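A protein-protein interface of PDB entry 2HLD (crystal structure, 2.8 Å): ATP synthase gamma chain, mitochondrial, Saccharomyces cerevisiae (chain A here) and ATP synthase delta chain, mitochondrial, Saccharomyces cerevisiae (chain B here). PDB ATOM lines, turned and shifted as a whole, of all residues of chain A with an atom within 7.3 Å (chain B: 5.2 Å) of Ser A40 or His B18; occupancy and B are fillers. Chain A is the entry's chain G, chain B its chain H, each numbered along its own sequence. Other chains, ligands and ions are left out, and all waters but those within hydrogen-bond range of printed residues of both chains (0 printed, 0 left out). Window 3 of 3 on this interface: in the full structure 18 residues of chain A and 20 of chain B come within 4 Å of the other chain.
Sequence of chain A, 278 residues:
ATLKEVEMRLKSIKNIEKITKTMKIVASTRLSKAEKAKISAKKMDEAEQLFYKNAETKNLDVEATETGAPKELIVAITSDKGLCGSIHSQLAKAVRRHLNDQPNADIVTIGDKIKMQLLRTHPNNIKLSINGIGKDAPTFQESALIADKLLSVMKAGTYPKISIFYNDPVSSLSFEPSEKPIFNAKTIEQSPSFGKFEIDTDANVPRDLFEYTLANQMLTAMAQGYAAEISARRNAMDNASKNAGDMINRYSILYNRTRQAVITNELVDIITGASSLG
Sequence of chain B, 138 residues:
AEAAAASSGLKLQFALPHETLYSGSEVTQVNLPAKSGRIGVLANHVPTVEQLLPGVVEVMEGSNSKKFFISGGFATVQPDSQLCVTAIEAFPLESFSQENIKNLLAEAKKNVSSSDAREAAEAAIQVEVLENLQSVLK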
ATOM      1  N   ALA A  34     -19.580 -21.697  29.883  1.00  0.00           N
ATOM      2  CA  ALA A  34     -19.470 -20.271  29.540  1.00  0.00           C
ATOM      3  C   ALA A  34     -18.442 -20.000  28.452  1.00  0.00           C
ATOM      4  O   ALA A  34     -18.507 -18.968  27.792  1.00  0.00           O
ATOM      5  CB  ALA A  34     -19.147 -19.440  30.780  1.00  0.00           C
ATOM      6  N   GLU A  35     -17.492 -20.914  28.275  1.00  0.00           N
ATOM      7  CA  GLU A  35     -16.536 -20.836  27.169  1.00  0.00           C
ATOM      8  C   GLU A  35     -17.201 -21.187  25.827  1.00  0.00           C
ATOM      9  O   GLU A  35     -16.774 -20.717  24.764  1.00  0.00           O
ATOM     10  CB  GLU A  35     -15.334 -21.747  27.434  1.00  0.00           C
ATOM     11  CG  GLU A  35     -14.432 -21.280  28.570  1.00  0.00           C
ATOM     12  CD  GLU A  35     -13.700 -19.978  28.265  1.00  0.00           C
ATOM     13  OE1 GLU A  35     -13.122 -19.853  27.161  1.00  0.00           O
ATOM     14  OE2 GLU A  35     -13.695 -19.079  29.134  1.00  0.00           O
ATOM     15  N   LYS A  36     -18.250 -22.008  25.897  1.00  0.00           N
ATOM     16  CA  LYS A  36     -19.057 -22.386  24.732  1.00  0.00           C
ATOM     17  C   LYS A  36     -20.020 -21.266  24.314  1.00  0.00           C
ATOM     18  O   LYS A  36     -20.312 -21.100  23.124  1.00  0.00           O
ATOM     19  CB  LYS A  36     -19.812 -23.694  25.009  1.00  0.00           C
ATOM     20  CG  LYS A  36     -18.876 -24.886  25.249  1.00  0.00           C
ATOM     21  CD  LYS A  36     -19.621 -26.198  25.460  1.00  0.00           C
ATOM     22  CE  LYS A  36     -18.649 -27.375  25.420  1.00  0.00           C
ATOM     23  NZ  LYS A  36     -19.351 -28.630  25.051  1.00  0.00           N
ATOM     24  N   ALA A  37     -20.503 -20.505  25.298  1.00  0.00           N
ATOM     25  CA  ALA A  37     -21.283 -19.294  25.043  1.00  0.00           C
ATOM     26  C   ALA A  37     -20.390 -18.124  24.621  1.00  0.00           C
ATOM     27  O   ALA A  37     -20.872 -17.167  24.016  1.00  0.00           O
ATOM     28  CB  ALA A  37     -22.111 -18.917  26.269  1.00  0.00           C
ATOM     29  N   LYS A  38     -19.098 -18.201  24.937  1.00  0.00           N
ATOM     30  CA  LYS A  38     -18.181 -17.099  24.646  1.00  0.00           C
ATOM     31  C   LYS A  38     -17.502 -17.243  23.292  1.00  0.00           C
ATOM     32  O   LYS A  38     -17.272 -16.246  22.605  1.00  0.00           O
ATOM     33  CB  LYS A  38     -17.130 -16.924  25.744  1.00  0.00           C
ATOM     34  CG  LYS A  38     -16.453 -15.563  25.712  1.00  0.00           C
ATOM     35  CD  LYS A  38     -15.070 -15.592  26.334  1.00  0.00           C
ATOM     36  CE  LYS A  38     -14.037 -16.198  25.397  1.00  0.00           C
ATOM     37  NZ  LYS A  38     -12.658 -15.813  25.812  1.00  0.00           N
ATOM     38  N   ILE A  39     -17.157 -18.474  22.921  1.00  0.00           N
ATOM     39  CA  ILE A  39     -16.620 -18.731  21.585  1.00  0.00           C
ATOM     40  C   ILE A  39     -17.703 -18.493  20.524  1.00  0.00           C
ATOM     41  O   ILE A  39     -17.443 -17.865  19.499  1.00  0.00           O
ATOM     42  CB  ILE A  39     -15.979 -20.157  21.490  1.00  0.00           C
ATOM     43  CG1 ILE A  39     -14.540 -20.156  22.055  1.00  0.00           C
ATOM     44  CG2 ILE A  39     -16.057 -20.735  20.052  1.00  0.00           C
ATOM     45  CD1 ILE A  39     -13.495 -19.318  21.269  1.00  0.00           C
ATOM     46  N   SER A  40     -18.920 -18.959  20.796  1.00  0.00           N
ATOM     47  CA  SER A  40     -20.040 -18.764  19.874  1.00  0.00           C
ATOM     48  C   SER A  40     -20.529 -17.312  19.748  1.00  0.00           C
ATOM     49  O   SER A  40     -21.234 -16.982  18.788  1.00  0.00           O
ATOM     50  CB  SER A  40     -21.203 -19.700  20.218  1.00  0.00           C
ATOM     51  OG  SER A  40     -21.041 -20.964  19.594  1.00  0.00           O
ATOM     52  N   ALA A  41     -20.156 -16.454  20.700  1.00  0.00           N
ATOM     53  CA  ALA A  41     -20.492 -15.023  20.640  1.00  0.00           C
ATOM     54  C   ALA A  41     -19.383 -14.153  20.035  1.00  0.00           C
ATOM     55  O   ALA A  41     -19.680 -13.167  19.370  1.00  0.00           O
ATOM     56  CB  ALA A  41     -20.901 -14.494  22.009  1.00  0.00           C
ATOM     57  N   LYS A  42     -18.120 -14.516  20.260  1.00  0.00           N
ATOM     58  CA  LYS A  42     -16.988 -13.782  19.672  1.00  0.00           C
ATOM     59  C   LYS A  42     -16.759 -14.075  18.182  1.00  0.00           C
ATOM     60  O   LYS A  42     -16.111 -13.284  17.489  1.00  0.00           O
ATOM     61  CB  LYS A  42     -15.697 -14.003  20.469  1.00  0.00           C
ATOM     62  CG  LYS A  42     -15.310 -12.839  21.388  1.00  0.00           C
ATOM     63  CD  LYS A  42     -14.063 -13.187  22.193  1.00  0.00           C
ATOM     64  CE  LYS A  42     -13.152 -11.985  22.364  1.00  0.00           C
ATOM     65  NZ  LYS A  42     -11.748 -12.407  22.622  1.00  0.00           N
ATOM     66  N   LYS A  43     -17.258 -15.218  17.702  1.00  0.00           N
ATOM     67  CA  LYS A  43     -17.235 -15.535  16.267  1.00  0.00           C
ATOM     68  C   LYS A  43     -18.287 -14.703  15.541  1.00  0.00           C
ATOM     69  O   LYS A  43     -18.023 -14.162  14.462  1.00  0.00           O
ATOM     70  CB  LYS A  43     -17.477 -17.031  16.004  1.00  0.00           C
ATOM     71  CG  LYS A  43     -16.299 -17.973  16.323  1.00  0.00           C
ATOM     72  CD  LYS A  43     -15.155 -17.886  15.303  1.00  0.00           C
ATOM     73  CE  LYS A  43     -14.039 -18.864  15.647  1.00  0.00           C
ATOM     74  NZ  LYS A  43     -12.774 -18.503  14.951  1.00  0.00           N
ATOM     75  N   MET A  44     -19.471 -14.603  16.145  1.00  0.00           N
ATOM     76  CA  MET A  44     -20.545 -13.752  15.632  1.00  0.00           C
ATOM     77  C   MET A  44     -20.192 -12.262  15.768  1.00  0.00           C
ATOM     78  O   MET A  44     -20.789 -11.403  15.119  1.00  0.00           O
ATOM     79  CB  MET A  44     -21.845 -14.050  16.368  1.00  0.00           C
ATOM     80  CG  MET A  44     -23.084 -13.640  15.621  1.00  0.00           C
ATOM     81  SD  MET A  44     -24.398 -13.554  16.811  1.00  0.00           S
ATOM     82  CE  MET A  44     -25.897 -13.589  15.833  1.00  0.00           C
ATOM     83  N   ASP A  45     -19.215 -11.978  16.623  1.00  0.00           N
ATOM     84  CA  ASP A  45     -18.705 -10.632  16.826  1.00  0.00           C
ATOM     85  C   ASP A  45     -17.784 -10.208  15.692  1.00  0.00           C
ATOM     86  O   ASP A  45     -17.680  -9.027  15.386  1.00  0.00           O
ATOM     87  CB  ASP A  45     -17.938 -10.563  18.138  1.00  0.00           C
ATOM     88  CG  ASP A  45     -17.838  -9.163  18.672  1.00  0.00           C
ATOM     89  OD1 ASP A  45     -18.867  -8.451  18.665  1.00  0.00           O
ATOM     90  OD2 ASP A  45     -16.775  -8.694  19.130  1.00  0.00           O
ATOM     91  N   PHE A 140     -29.650 -13.928  24.188  1.00  0.00           N
ATOM     92  CA  PHE A 140     -30.221 -12.947  23.266  1.00  0.00           C
ATOM     93  C   PHE A 140     -31.561 -12.388  23.716  1.00  0.00           C
ATOM     94  O   PHE A 140     -31.873 -11.232  23.450  1.00  0.00           O
ATOM     95  CB  PHE A 140     -30.351 -13.512  21.840  1.00  0.00           C
ATOM     96  CG  PHE A 140     -30.590 -12.454  20.793  1.00  0.00           C
ATOM     97  CD1 PHE A 140     -31.883 -12.015  20.502  1.00  0.00           C
ATOM     98  CD2 PHE A 140     -29.512 -11.861  20.124  1.00  0.00           C
ATOM     99  CE1 PHE A 140     -32.094 -11.019  19.561  1.00  0.00           C
ATOM    100  CE2 PHE A 140     -29.715 -10.861  19.177  1.00  0.00           C
ATOM    101  CZ  PHE A 140     -31.008 -10.447  18.890  1.00  0.00           C
ATOM    102  N   LEU A 219     -25.064  -8.516  23.995  1.00  0.00           N
ATOM    103  CA  LEU A 219     -24.923  -9.948  24.264  1.00  0.00           C
ATOM    104  C   LEU A 219     -23.460 -10.361  24.285  1.00  0.00           C
ATOM    105  O   LEU A 219     -23.004 -11.058  25.184  1.00  0.00           O
ATOM    106  CB  LEU A 219     -25.684 -10.793  23.232  1.00  0.00           C
ATOM    107  CG  LEU A 219     -25.623 -12.315  23.452  1.00  0.00           C
ATOM    108  CD1 LEU A 219     -26.919 -12.976  23.056  1.00  0.00           C
ATOM    109  CD2 LEU A 219     -24.468 -12.951  22.696  1.00  0.00           C
ATOM    110  N   THR A 220     -22.729  -9.932  23.277  1.00  0.00           N
ATOM    111  CA  THR A 220     -21.328 -10.269  23.171  1.00  0.00           C
ATOM    112  C   THR A 220     -20.556  -9.827  24.414  1.00  0.00           C
ATOM    113  O   THR A 220     -19.706 -10.555  24.895  1.00  0.00           O
ATOM    114  CB  THR A 220     -20.766  -9.657  21.877  1.00  0.00           C
ATOM    115  OG1 THR A 220     -21.508 -10.193  20.773  1.00  0.00           O
ATOM    116  CG2 THR A 220     -19.351 -10.115  21.608  1.00  0.00           C
ATOM    117  N   LEU B  16     -24.466 -18.242  14.692  1.00  0.00           N
ATOM    118  CA  LEU B  16     -25.576 -17.947  15.601  1.00  0.00           C
ATOM    119  C   LEU B  16     -24.978 -17.581  16.974  1.00  0.00           C
ATOM    120  O   LEU B  16     -23.775 -17.824  17.191  1.00  0.00           O
ATOM    121  CB  LEU B  16     -26.550 -19.128  15.677  1.00  0.00           C
ATOM    122  N   PRO B  17     -25.771 -16.972  17.875  1.00  0.00           N
ATOM    123  CA  PRO B  17     -25.242 -16.518  19.172  1.00  0.00           C
ATOM    124  C   PRO B  17     -24.746 -17.685  20.008  1.00  0.00           C
ATOM    125  O   PRO B  17     -23.646 -17.607  20.564  1.00  0.00           O
ATOM    126  CB  PRO B  17     -26.442 -15.815  19.843  1.00  0.00           C
ATOM    127  CG  PRO B  17     -27.651 -16.284  19.124  1.00  0.00           C
ATOM    128  CD  PRO B  17     -27.206 -16.658  17.739  1.00  0.00           C
ATOM    129  N   HIS B  18     -25.546 -18.759  20.043  1.00  0.00           N
ATOM    130  CA  HIS B  18     -25.235 -20.008  20.762  1.00  0.00           C
ATOM    131  C   HIS B  18     -24.399 -21.043  19.999  1.00  0.00           C
ATOM    132  O   HIS B  18     -23.654 -21.800  20.616  1.00  0.00           O
ATOM    133  CB  HIS B  18     -26.516 -20.668  21.284  1.00  0.00           C
ATOM    134  CG  HIS B  18     -27.563 -20.895  20.238  1.00  0.00           C
ATOM    135  ND1 HIS B  18     -27.486 -21.919  19.319  1.00  0.00           N
ATOM    136  CD2 HIS B  18     -28.728 -20.250  19.988  1.00  0.00           C
ATOM    137  CE1 HIS B  18     -28.554 -21.889  18.540  1.00  0.00           C
ATOM    138  NE2 HIS B  18     -29.325 -20.889  18.929  1.00  0.00           N
ATOM    139  N   GLU B  19     -24.524 -21.096  18.678  1.00  0.00           N
ATOM    140  CA  GLU B  19     -23.692 -21.997  17.882  1.00  0.00           C
ATOM    141  C   GLU B  19     -23.232 -21.390  16.548  1.00  0.00           C
ATOM    142  O   GLU B  19     -24.050 -20.911  15.756  1.00  0.00           O
ATOM    143  CB  GLU B  19     -24.390 -23.361  17.678  1.00  0.00           C
ATOM    144  CG  GLU B  19     -23.507 -24.449  17.064  1.00  0.00           C
ATOM    145  CD  GLU B  19     -22.236 -24.713  17.866  1.00  0.00           C
ATOM    146  OE1 GLU B  19     -22.296 -25.502  18.838  1.00  0.00           O
ATOM    147  OE2 GLU B  19     -21.172 -24.139  17.526  1.00  0.00           O
ATOM    148  N   THR B  20     -21.919 -21.413  16.312  1.00  0.00           N
ATOM    149  CA  THR B  20     -21.377 -21.047  15.004  1.00  0.00           C
ATOM    150  C   THR B  20     -21.531 -22.235  14.051  1.00  0.00           C
ATOM    151  O   THR B  20     -21.130 -23.354  14.377  1.00  0.00           O
ATOM    152  CB  THR B  20     -19.888 -20.584  15.088  1.00  0.00           C
ATOM    153  OG1 THR B  20     -19.017 -21.717  15.157  1.00  0.00           O
ATOM    154  CG2 THR B  20     -19.611 -19.853  16.382  1.00  0.00           C
ATOM    155  N   ILE B  88     -30.418 -15.616  15.091  1.00  0.00           N
ATOM    156  CA  ILE B  88     -30.550 -16.163  16.449  1.00  0.00           C
ATOM    157  C   ILE B  88     -30.707 -17.702  16.426  1.00  0.00           C
ATOM    158  O   ILE B  88     -29.836 -18.442  16.909  1.00  0.00           O
ATOM    159  CB  ILE B  88     -31.727 -15.504  17.226  1.00  0.00           C
ATOM    160  CG1 ILE B  88     -31.757 -13.989  17.008  1.00  0.00           C
ATOM    161  CG2 ILE B  88     -31.638 -15.847  18.715  1.00  0.00           C
ATOM    162  CD1 ILE B  88     -33.120 -13.378  17.253  1.00  0.00           C
ATOM    163  N   GLU B  89     -31.818 -18.166  15.855  1.00  0.00           N
ATOM    164  CA  GLU B  89     -32.105 -19.591  15.779  1.00  0.00           C
ATOM    165  C   GLU B  89     -31.803 -20.132  14.386  1.00  0.00           C
ATOM    166  O   GLU B  89     -32.231 -19.551  13.383  1.00  0.00           O
ATOM    167  CB  GLU B  89     -33.560 -19.887  16.189  1.00  0.00           C
ATOM    168  CG  GLU B  89     -33.853 -19.774  17.692  1.00  0.00           C
ATOM    169  CD  GLU B  89     -32.805 -20.452  18.584  1.00  0.00           C
ATOM    170  OE1 GLU B  89     -32.335 -21.564  18.254  1.00  0.00           O
ATOM    171  OE2 GLU B  89     -32.438 -19.868  19.629  1.00  0.00           O
ATOM    172  N   ALA B  90     -31.046 -21.231  14.338  1.00  0.00           N
ATOM    173  CA  ALA B  90     -30.763 -21.938  13.081  1.00  0.00           C
ATOM    174  C   ALA B  90     -30.869 -23.462  13.236  1.00  0.00           C
ATOM    175  O   ALA B  90     -29.864 -24.167  13.395  1.00  0.00           O
ATOM    176  CB  ALA B  90     -29.397 -21.537  12.535  1.00  0.00           C
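Glu B19 touches Ser A40 (CA to OG, 3.3 Å). N of Ala A41 touches O of Pro B17, at 3.7 Å. Thr B20 touches Lys A43 (CG2 to CB, 3.6 Å). Met A44 touches Pro B17 (SD to N, 3.8 Å). Ile B88 touches Phe A140 (CD1 to CE1, 3.5 Å).
NE2 of His B18 is in hydrogen-bond range of OE1 of Glu B89, 3.2 Å away. NE2 of His B18 sits at hydrogen-bond distance from O of Ile B88.
Of chain A, only Ser A40 (2.9 Å) comes within 4 Å of His B18. Of the printed residues of chain A, Pro B17 touches Ser A40 (3.1 Å), Ala A41 (3.7 Å) and Met A44 (3.8 Å). Of the printed residues of chain B, Met A44 touches Pro B17 (3.8 Å). Printed residues of chain B within 4 Å of Ala A41: Pro B17. Of the printed residues of chain A, Ile B88 touches Phe A140 (3.5 Å). Ala A37 touches none of the printed residues of chain B. Ala B90 touches none of the printed residues of chain A. The nearest printed residue of chain B that does not touch Ser A40 is Ile B88 (8.9 Å).
The backbone carbonyl oxygen of Ser A40 sits close to the backbone carbonyl oxygen of Pro B17. OG of Ser A40 is in hydrogen-bond range of O of His B18, 2.9 Å away. The backbone NH (N) of Thr B20 sits at hydrogen-bond distance from the side-chain hydroxyl (OG) of Ser A40. The backbone carbonyl oxygen of Ser A40 sits close to the backbone carbonyl oxygen of Leu B16, 3.1 Å away.
Hydrophobic or aromatic side chains of chain A within 4 Å of the printed part of chain B: Met A44 and Phe A140. Of the 8 printed residues of chain B, 6 touch a printed residue of chain A. Printed residues of chain B that touch a printed residue of chain A: Leu B16, Pro B17, His B18, Glu B19, Thr B20 and Ile B88. Hydrophobic or aromatic side chains of chain B that line the printed part of chain A: Pro B17 and Ile B88. Among the printed residues, 9 pairs touch across the chains.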
